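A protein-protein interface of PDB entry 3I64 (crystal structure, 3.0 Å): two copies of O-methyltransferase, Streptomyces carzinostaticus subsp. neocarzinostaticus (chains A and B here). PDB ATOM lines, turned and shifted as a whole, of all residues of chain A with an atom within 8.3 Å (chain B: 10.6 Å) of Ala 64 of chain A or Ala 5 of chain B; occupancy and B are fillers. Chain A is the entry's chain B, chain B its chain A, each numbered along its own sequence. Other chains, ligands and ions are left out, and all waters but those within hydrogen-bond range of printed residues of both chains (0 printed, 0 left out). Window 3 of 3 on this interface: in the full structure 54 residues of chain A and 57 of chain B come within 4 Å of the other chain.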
ATOM      1  N   ILE A   8     -14.461  36.353  13.996  1.00  0.00           N
ATOM      2  CA  ILE A   8     -13.564  35.464  14.726  1.00  0.00           C
ATOM      3  C   ILE A   8     -13.365  36.128  16.085  1.00  0.00           C
ATOM      4  O   ILE A   8     -13.521  37.339  16.232  1.00  0.00           O
ATOM      5  CB  ILE A   8     -12.339  35.082  13.877  1.00  0.00           C
ATOM      6  CG1 ILE A   8     -12.127  36.102  12.757  1.00  0.00           C
ATOM      7  CG2 ILE A   8     -12.505  33.684  13.304  1.00  0.00           C
ATOM      8  CD1 ILE A   8     -13.379  36.411  11.968  1.00  0.00           C
ATOM      9  N   THR A  18      -0.092  33.506  14.830  1.00  0.00           N
ATOM     10  CA  THR A  18      -0.299  32.978  13.490  1.00  0.00           C
ATOM     11  C   THR A  18       0.341  33.800  12.378  1.00  0.00           C
ATOM     12  O   THR A  18       1.121  33.268  11.587  1.00  0.00           O
ATOM     13  CB  THR A  18      -1.807  32.767  13.203  1.00  0.00           C
ATOM     14  OG1 THR A  18      -2.217  31.538  13.805  1.00  0.00           O
ATOM     15  CG2 THR A  18      -2.090  32.700  11.710  1.00  0.00           C
ATOM     16  N   ARG A  57       6.996  22.421  15.993  1.00  0.00           N
ATOM     17  CA  ARG A  57       5.911  23.105  16.682  1.00  0.00           C
ATOM     18  C   ARG A  57       5.298  24.192  15.797  1.00  0.00           C
ATOM     19  O   ARG A  57       4.085  24.418  15.830  1.00  0.00           O
ATOM     20  CB  ARG A  57       6.445  23.694  17.990  1.00  0.00           C
ATOM     21  CG  ARG A  57       7.563  22.843  18.584  1.00  0.00           C
ATOM     22  CD  ARG A  57       7.520  22.769  20.094  1.00  0.00           C
ATOM     23  NE  ARG A  57       7.581  24.082  20.725  1.00  0.00           N
ATOM     24  CZ  ARG A  57       7.706  24.273  22.034  1.00  0.00           C
ATOM     25  NH1 ARG A  57       7.787  23.234  22.846  1.00  0.00           N
ATOM     26  NH2 ARG A  57       7.743  25.498  22.538  1.00  0.00           N
ATOM     27  N   LEU A  58       6.138  24.857  15.004  1.00  0.00           N
ATOM     28  CA  LEU A  58       5.682  25.904  14.090  1.00  0.00           C
ATOM     29  C   LEU A  58       4.747  25.300  13.047  1.00  0.00           C
ATOM     30  O   LEU A  58       3.618  25.773  12.844  1.00  0.00           O
ATOM     31  CB  LEU A  58       6.871  26.545  13.368  1.00  0.00           C
ATOM     32  CG  LEU A  58       6.541  27.573  12.277  1.00  0.00           C
ATOM     33  CD1 LEU A  58       5.776  28.740  12.866  1.00  0.00           C
ATOM     34  CD2 LEU A  58       7.815  28.070  11.650  1.00  0.00           C
ATOM     35  N   LEU A  59       5.236  24.249  12.389  1.00  0.00           N
ATOM     36  CA  LEU A  59       4.478  23.547  11.360  1.00  0.00           C
ATOM     37  C   LEU A  59       3.128  23.071  11.882  1.00  0.00           C
ATOM     38  O   LEU A  59       2.096  23.311  11.258  1.00  0.00           O
ATOM     39  CB  LEU A  59       5.297  22.364  10.829  1.00  0.00           C
ATOM     40  CG  LEU A  59       6.586  22.790  10.118  1.00  0.00           C
ATOM     41  CD1 LEU A  59       7.383  21.564   9.712  1.00  0.00           C
ATOM     42  CD2 LEU A  59       6.244  23.652   8.908  1.00  0.00           C
ATOM     43  N   ARG A  60       3.138  22.400  13.027  1.00  0.00           N
ATOM     44  CA  ARG A  60       1.906  21.909  13.630  1.00  0.00           C
ATOM     45  C   ARG A  60       0.864  23.025  13.700  1.00  0.00           C
ATOM     46  O   ARG A  60      -0.312  22.822  13.379  1.00  0.00           O
ATOM     47  CB  ARG A  60       2.186  21.419  15.035  1.00  0.00           C
ATOM     48  CG  ARG A  60       3.312  20.429  15.125  1.00  0.00           C
ATOM     49  CD  ARG A  60       2.816  19.023  14.961  1.00  0.00           C
ATOM     50  NE  ARG A  60       3.655  18.116  15.731  1.00  0.00           N
ATOM     51  CZ  ARG A  60       3.300  16.883  16.074  1.00  0.00           C
ATOM     52  NH1 ARG A  60       4.132  16.124  16.782  1.00  0.00           N
ATOM     53  NH2 ARG A  60       2.110  16.411  15.710  1.00  0.00           N
ATOM     54  N   HIS A  61       1.300  24.205  14.135  1.00  0.00           N
ATOM     55  CA  HIS A  61       0.400  25.346  14.236  1.00  0.00           C
ATOM     56  C   HIS A  61      -0.090  25.730  12.839  1.00  0.00           C
ATOM     57  O   HIS A  61      -1.247  26.108  12.643  1.00  0.00           O
ATOM     58  CB  HIS A  61       1.114  26.541  14.878  1.00  0.00           C
ATOM     59  CG  HIS A  61       0.270  27.776  14.927  1.00  0.00           C
ATOM     60  ND1 HIS A  61      -0.853  27.875  15.719  1.00  0.00           N
ATOM     61  CD2 HIS A  61       0.337  28.927  14.222  1.00  0.00           C
ATOM     62  CE1 HIS A  61      -1.444  29.034  15.495  1.00  0.00           C
ATOM     63  NE2 HIS A  61      -0.743  29.692  14.590  1.00  0.00           N
ATOM     64  N   LEU A  62       0.808  25.624  11.869  1.00  0.00           N
ATOM     65  CA  LEU A  62       0.480  25.953  10.492  1.00  0.00           C
ATOM     66  C   LEU A  62      -0.379  24.893   9.778  1.00  0.00           C
ATOM     67  O   LEU A  62      -1.041  25.206   8.784  1.00  0.00           O
ATOM     68  CB  LEU A  62       1.769  26.235   9.711  1.00  0.00           C
ATOM     69  CG  LEU A  62       2.378  27.595  10.057  1.00  0.00           C
ATOM     70  CD1 LEU A  62       3.628  27.843   9.244  1.00  0.00           C
ATOM     71  CD2 LEU A  62       1.354  28.677   9.776  1.00  0.00           C
ATOM     72  N   VAL A  63      -0.373  23.648  10.256  1.00  0.00           N
ATOM     73  CA  VAL A  63      -1.221  22.649   9.613  1.00  0.00           C
ATOM     74  C   VAL A  63      -2.619  22.969  10.131  1.00  0.00           C
ATOM     75  O   VAL A  63      -3.621  22.813   9.420  1.00  0.00           O
ATOM     76  CB  VAL A  63      -0.865  21.189   9.999  1.00  0.00           C
ATOM     77  CG1 VAL A  63       0.603  20.915   9.756  1.00  0.00           C
ATOM     78  CG2 VAL A  63      -1.240  20.927  11.428  1.00  0.00           C
ATOM     79  N   ALA A  64      -2.666  23.440  11.375  1.00  0.00           N
ATOM     80  CA  ALA A  64      -3.914  23.814  12.028  1.00  0.00           C
ATOM     81  C   ALA A  64      -4.553  25.017  11.327  1.00  0.00           C
ATOM     82  O   ALA A  64      -5.773  25.105  11.209  1.00  0.00           O
ATOM     83  CB  ALA A  64      -3.647  24.141  13.484  1.00  0.00           C
ATOM     84  N   VAL A  65      -3.720  25.947  10.873  1.00  0.00           N
ATOM     85  CA  VAL A  65      -4.209  27.133  10.183  1.00  0.00           C
ATOM     86  C   VAL A  65      -4.787  26.697   8.840  1.00  0.00           C
ATOM     87  O   VAL A  65      -5.745  27.287   8.333  1.00  0.00           O
ATOM     88  CB  VAL A  65      -3.064  28.133   9.919  1.00  0.00           C
ATOM     89  CG1 VAL A  65      -3.622  29.448   9.395  1.00  0.00           C
ATOM     90  CG2 VAL A  65      -2.257  28.340  11.183  1.00  0.00           C
ATOM     91  N   GLY A  66      -4.185  25.655   8.270  1.00  0.00           N
ATOM     92  CA  GLY A  66      -4.632  25.141   6.988  1.00  0.00           C
ATOM     93  C   GLY A  66      -3.643  25.400   5.871  1.00  0.00           C
ATOM     94  O   GLY A  66      -4.024  25.571   4.713  1.00  0.00           O
ATOM     95  N   LEU A  67      -2.364  25.441   6.209  1.00  0.00           N
ATOM     96  CA  LEU A  67      -1.354  25.680   5.201  1.00  0.00           C
ATOM     97  C   LEU A  67      -0.597  24.408   4.892  1.00  0.00           C
ATOM     98  O   LEU A  67      -0.065  24.251   3.799  1.00  0.00           O
ATOM     99  CB  LEU A  67      -0.375  26.763   5.659  1.00  0.00           C
ATOM    100  CG  LEU A  67      -0.868  28.209   5.657  1.00  0.00           C
ATOM    101  CD1 LEU A  67       0.311  29.122   5.958  1.00  0.00           C
ATOM    102  CD2 LEU A  67      -1.477  28.568   4.307  1.00  0.00           C
ATOM    103  N   PHE A  68      -0.541  23.500   5.858  1.00  0.00           N
ATOM    104  CA  PHE A  68       0.161  22.242   5.661  1.00  0.00           C
ATOM    105  C   PHE A  68      -0.671  21.078   6.167  1.00  0.00           C
ATOM    106  O   PHE A  68      -1.663  21.269   6.876  1.00  0.00           O
ATOM    107  CB  PHE A  68       1.508  22.234   6.400  1.00  0.00           C
ATOM    108  CG  PHE A  68       2.427  23.349   6.010  1.00  0.00           C
ATOM    109  CD1 PHE A  68       2.668  23.636   4.674  1.00  0.00           C
ATOM    110  CD2 PHE A  68       3.049  24.122   6.983  1.00  0.00           C
ATOM    111  CE1 PHE A  68       3.517  24.682   4.313  1.00  0.00           C
ATOM    112  CE2 PHE A  68       3.899  25.168   6.630  1.00  0.00           C
ATOM    113  CZ  PHE A  68       4.134  25.450   5.294  1.00  0.00           C
ATOM    114  N   THR A  69      -0.248  19.876   5.789  1.00  0.00           N
ATOM    115  CA  THR A  69      -0.898  18.638   6.193  1.00  0.00           C
ATOM    116  C   THR A  69       0.201  17.767   6.757  1.00  0.00           C
ATOM    117  O   THR A  69       1.334  17.805   6.283  1.00  0.00           O
ATOM    118  CB  THR A  69      -1.525  17.898   5.000  1.00  0.00           C
ATOM    119  OG1 THR A  69      -0.486  17.402   4.145  1.00  0.00           O
ATOM    120  CG2 THR A  69      -2.427  18.832   4.207  1.00  0.00           C
ATOM    121  N   ARG A  70      -0.133  16.982   7.770  1.00  0.00           N
ATOM    122  CA  ARG A  70       0.843  16.104   8.401  1.00  0.00           C
ATOM    123  C   ARG A  70       0.165  14.778   8.712  1.00  0.00           C
ATOM    124  O   ARG A  70      -1.018  14.744   9.066  1.00  0.00           O
ATOM    125  CB  ARG A  70       1.384  16.771   9.675  1.00  0.00           C
ATOM    126  CG  ARG A  70       2.324  15.932  10.516  1.00  0.00           C
ATOM    127  CD  ARG A  70       1.547  15.135  11.554  1.00  0.00           C
ATOM    128  NE  ARG A  70       2.405  14.342  12.433  1.00  0.00           N
ATOM    129  CZ  ARG A  70       3.469  14.819  13.074  1.00  0.00           C
ATOM    130  NH1 ARG A  70       3.823  16.094  12.935  1.00  0.00           N
ATOM    131  NH2 ARG A  70       4.168  14.024  13.871  1.00  0.00           N
ATOM    132  N   TYR A  76       4.995  16.082   6.195  1.00  0.00           N
ATOM    133  CA  TYR A  76       4.267  17.294   5.854  1.00  0.00           C
ATOM    134  C   TYR A  76       4.031  17.482   4.367  1.00  0.00           C
ATOM    135  O   TYR A  76       4.857  17.099   3.542  1.00  0.00           O
ATOM    136  CB  TYR A  76       4.986  18.524   6.427  1.00  0.00           C
ATOM    137  CG  TYR A  76       5.008  18.572   7.945  1.00  0.00           C
ATOM    138  CD1 TYR A  76       6.065  18.015   8.665  1.00  0.00           C
ATOM    139  CD2 TYR A  76       3.957  19.145   8.661  1.00  0.00           C
ATOM    140  CE1 TYR A  76       6.076  18.021  10.058  1.00  0.00           C
ATOM    141  CE2 TYR A  76       3.958  19.158  10.060  1.00  0.00           C
ATOM    142  CZ  TYR A  76       5.022  18.592  10.749  1.00  0.00           C
ATOM    143  OH  TYR A  76       5.036  18.593  12.125  1.00  0.00           O
ATOM    144  N   THR A  79      -1.023  22.252   1.387  1.00  0.00           N
ATOM    145  CA  THR A  79      -2.437  22.086   1.111  1.00  0.00           C
ATOM    146  C   THR A  79      -2.678  22.986  -0.080  1.00  0.00           C
ATOM    147  O   THR A  79      -1.765  23.680  -0.525  1.00  0.00           O
ATOM    148  CB  THR A  79      -3.328  22.569   2.276  1.00  0.00           C
ATOM    149  OG1 THR A  79      -3.149  23.978   2.467  1.00  0.00           O
ATOM    150  CG2 THR A  79      -2.980  21.840   3.557  1.00  0.00           C
ATOM    151  N   ALA B   5      -8.238  25.051   8.916  1.00  0.00           N
ATOM    152  CA  ALA B   5      -9.533  25.789   9.007  1.00  0.00           C
ATOM    153  C   ALA B   5      -9.339  27.308   8.930  1.00  0.00           C
ATOM    154  O   ALA B   5      -9.543  28.023   9.913  1.00  0.00           O
ATOM    155  CB  ALA B   5     -10.255  25.415  10.302  1.00  0.00           C
ATOM    156  N   ALA B   6      -8.939  27.789   7.755  1.00  0.00           N
ATOM    157  CA  ALA B   6      -8.722  29.215   7.506  1.00  0.00           C
ATOM    158  C   ALA B   6      -8.566  29.405   5.998  1.00  0.00           C
ATOM    159  O   ALA B   6      -7.479  29.261   5.430  1.00  0.00           O
ATOM    160  CB  ALA B   6      -7.482  29.706   8.241  1.00  0.00           C
ATOM    161  N   HIS B   7      -9.675  29.752   5.355  1.00  0.00           N
ATOM    162  CA  HIS B   7      -9.712  29.918   3.909  1.00  0.00           C
ATOM    163  C   HIS B   7      -9.299  31.315   3.458  1.00  0.00           C
ATOM    164  O   HIS B   7      -8.897  31.502   2.310  1.00  0.00           O
ATOM    165  CB  HIS B   7     -11.111  29.597   3.383  1.00  0.00           C
ATOM    166  CG  HIS B   7     -12.188  29.739   4.412  1.00  0.00           C
ATOM    167  ND1 HIS B   7     -12.122  30.661   5.434  1.00  0.00           N
ATOM    168  CD2 HIS B   7     -13.356  29.075   4.580  1.00  0.00           C
ATOM    169  CE1 HIS B   7     -13.203  30.560   6.187  1.00  0.00           C
ATOM    170  NE2 HIS B   7     -13.968  29.605   5.690  1.00  0.00           N
ATOM    171  N   ILE B   8      -9.399  32.296   4.350  1.00  0.00           N
ATOM    172  CA  ILE B   8      -9.072  33.673   3.974  1.00  0.00           C
ATOM    173  C   ILE B   8      -7.662  33.776   3.393  1.00  0.00           C
ATOM    174  O   ILE B   8      -6.766  33.021   3.779  1.00  0.00           O
ATOM    175  CB  ILE B   8      -9.212  34.637   5.180  1.00  0.00           C
ATOM    176  CG1 ILE B   8      -8.376  34.140   6.363  1.00  0.00           C
ATOM    177  CG2 ILE B   8     -10.673  34.744   5.585  1.00  0.00           C
ATOM    178  CD1 ILE B   8      -8.570  34.953   7.642  1.00  0.00           C
ATOM    179  N   GLY B   9      -7.481  34.710   2.462  1.00  0.00           N
ATOM    180  CA  GLY B   9      -6.194  34.903   1.804  1.00  0.00           C
ATOM    181  C   GLY B   9      -4.866  34.917   2.544  1.00  0.00           C
ATOM    182  O   GLY B   9      -4.721  35.555   3.588  1.00  0.00           O
ATOM    183  N   LEU B  13      -3.816  36.279   6.161  1.00  0.00           N
ATOM    184  CA  LEU B  13      -3.447  35.366   7.230  1.00  0.00           C
ATOM    185  C   LEU B  13      -2.186  35.871   7.940  1.00  0.00           C
ATOM    186  O   LEU B  13      -2.047  35.764   9.164  1.00  0.00           O
ATOM    187  CB  LEU B  13      -3.166  33.982   6.649  1.00  0.00           C
ATOM    188  CG  LEU B  13      -3.996  32.766   7.058  1.00  0.00           C
ATOM    189  CD1 LEU B  13      -3.178  31.523   6.734  1.00  0.00           C
ATOM    190  CD2 LEU B  13      -4.327  32.788   8.544  1.00  0.00           C
ATOM    191  N   ALA B 282      -5.721  24.299  25.579  1.00  0.00           N
ATOM    192  CA  ALA B 282      -4.358  24.126  25.123  1.00  0.00           C
ATOM    193  C   ALA B 282      -4.380  24.004  23.607  1.00  0.00           C
ATOM    194  O   ALA B 282      -5.193  23.280  23.034  1.00  0.00           O
ATOM    195  CB  ALA B 282      -3.741  22.888  25.750  1.00  0.00           C
ATOM    196  N   GLY B 283      -3.470  24.730  22.973  1.00  0.00           N
ATOM    197  CA  GLY B 283      -3.337  24.755  21.526  1.00  0.00           C
ATOM    198  C   GLY B 283      -1.932  25.031  21.040  1.00  0.00           C
ATOM    199  O   GLY B 283      -1.037  25.304  21.833  1.00  0.00           O
ATOM    200  N   THR B 284      -1.732  24.954  19.728  1.00  0.00           N
ATOM    201  CA  THR B 284      -0.426  25.215  19.139  1.00  0.00           C
ATOM    202  C   THR B 284      -0.042  26.680  19.371  1.00  0.00           C
ATOM    203  O   THR B 284       1.136  27.004  19.508  1.00  0.00           O
ATOM    204  CB  THR B 284      -0.416  24.906  17.618  1.00  0.00           C
ATOM    205  OG1 THR B 284      -1.468  25.626  16.964  1.00  0.00           O
ATOM    206  CG2 THR B 284      -0.610  23.426  17.377  1.00  0.00           C
ATOM    207  N   GLY B 285      -1.040  27.559  19.419  1.00  0.00           N
ATOM    208  CA  GLY B 285      -0.777  28.968  19.661  1.00  0.00           C
ATOM    209  C   GLY B 285      -0.280  29.162  21.084  1.00  0.00           C
ATOM    210  O   GLY B 285       0.532  30.046  21.364  1.00  0.00           O
ATOM    211  N   MET B 286      -0.776  28.337  21.999  1.00  0.00           N
ATOM    212  CA  MET B 286      -0.332  28.434  23.374  1.00  0.00           C
ATOM    213  C   MET B 286       1.105  27.934  23.393  1.00  0.00           C
ATOM    214  O   MET B 286       1.997  28.601  23.921  1.00  0.00           O
ATOM    215  CB  MET B 286      -1.213  27.586  24.299  1.00  0.00           C
ATOM    216  CG  MET B 286      -0.833  27.651  25.805  1.00  0.00           C
ATOM    217  SD  MET B 286      -0.524  29.337  26.608  1.00  0.00           S
ATOM    218  CE  MET B 286      -1.610  30.504  25.595  1.00  0.00           C
ATOM    219  N   ASP B 287       1.327  26.771  22.787  1.00  0.00           N
ATOM    220  CA  ASP B 287       2.657  26.180  22.731  1.00  0.00           C
ATOM    221  C   ASP B 287       3.675  27.129  22.101  1.00  0.00           C
ATOM    222  O   ASP B 287       4.827  27.187  22.526  1.00  0.00           O
ATOM    223  CB  ASP B 287       2.614  24.865  21.951  1.00  0.00           C
ATOM    224  CG  ASP B 287       3.968  24.186  21.882  1.00  0.00           C
ATOM    225  OD1 ASP B 287       4.517  23.836  22.948  1.00  0.00           O
ATOM    226  OD2 ASP B 287       4.484  24.005  20.761  1.00  0.00           O
ATOM    227  N   LEU B 288       3.258  27.868  21.079  1.00  0.00           N
ATOM    228  CA  LEU B 288       4.167  28.807  20.442  1.00  0.00           C
ATOM    229  C   LEU B 288       4.489  29.922  21.423  1.00  0.00           C
ATOM    230  O   LEU B 288       5.647  30.344  21.537  1.00  0.00           O
ATOM    231  CB  LEU B 288       3.556  29.387  19.165  1.00  0.00           C
ATOM    232  CG  LEU B 288       3.510  28.402  17.994  1.00  0.00           C
ATOM    233  CD1 LEU B 288       3.158  29.160  16.721  1.00  0.00           C
ATOM    234  CD2 LEU B 288       4.860  27.704  17.841  1.00  0.00           C
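The backbone NH (N) of Ala 5 of chain B is in hydrogen-bond range of the backbone carbonyl oxygen (O) of Ala 64 of chain A (3.4 Å).
The backbone carbonyl oxygen (O) of Val 65 of chain A is in hydrogen-bond range of the backbone NH (N) of Ala 5 of chain B (3.4 Å).
The backbone NH (N) of Ala 6 of chain B lies close to the backbone carbonyl oxygen (O) of Val 65 of chain A (3.3 Å).
OG1 of Thr 284 of chain B is in hydrogen-bond range of ND1 of His 61 of chain A (2.6 Å).
The side-chain carboxylate (OD2) of Asp 287 of chain B lies within salt-bridge range of the guanidinium group (NE) of Arg 57 of chain A, at 3.1 Å.
The side-chain hydroxyl of Thr 18 of chain A lies within hydrogen-bond range of a ring nitrogen (NE2) of His 61 of chain A, 2.5 Å away.
Thr 18 of chain A touches Leu 13 of chain B.
Leu 288 of chain B touches Arg 57 of chain A.
Thr 284 of chain B touches Arg 60 of chain A (CG2 to C, 3.98 Å).
Gly 285 of chain B touches His 61 of chain A (N to ND1, 3.7 Å).
CD1 of Leu 288 of chain B touches CG of His 61 of chain A (3.7 Å).
CG1 of Val 65 of chain A touches CD1 of Leu 13 of chain B (3.4 Å).
Of the printed residues of chain B, Arg 57 of chain A touches Asp 287 and Leu 288.
Of the printed residues of chain B, Val 65 of chain A touches Ala 5 (3.4 Å), Ala 6 (3.0 Å) and Leu 13 (3.4 Å).
No residue of chain B comes within 4 Å of Gly 66 of chain A.
Leu 67 of chain A touches none of the printed residues of chain B.
Of the printed residues of chain A, Ala 5 of chain B touches Ala 64 (3.4 Å) and Val 65 (3.4 Å).
Of the printed residues of chain A, Leu 13 of chain B touches Thr 18 (3.9 Å) and Val 65 (3.4 Å).
The nearest residue of chain B that does not touch Ala 64 of chain A is Thr 284 of chain B (4.4 Å).
Of the 18 printed residues of chain A, 6 touch a printed residue of chain B.
Hydrophobic or aromatic side chains of chain A that line the printed part of chain B: His 61 and Val 65.
Of the 13 printed residues of chain B, 7 touch a printed residue of chain A.
Among the printed residues, 11 pairs touch across the chains.
Among the printed residues, Asp or Glu carboxylates within 4 Å of a Lys or Arg side-chain nitrogen of the other chain: Arg 57 of chain A with Asp 287 of chain B (3.1 Å).
Position printed for both chains: 8.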
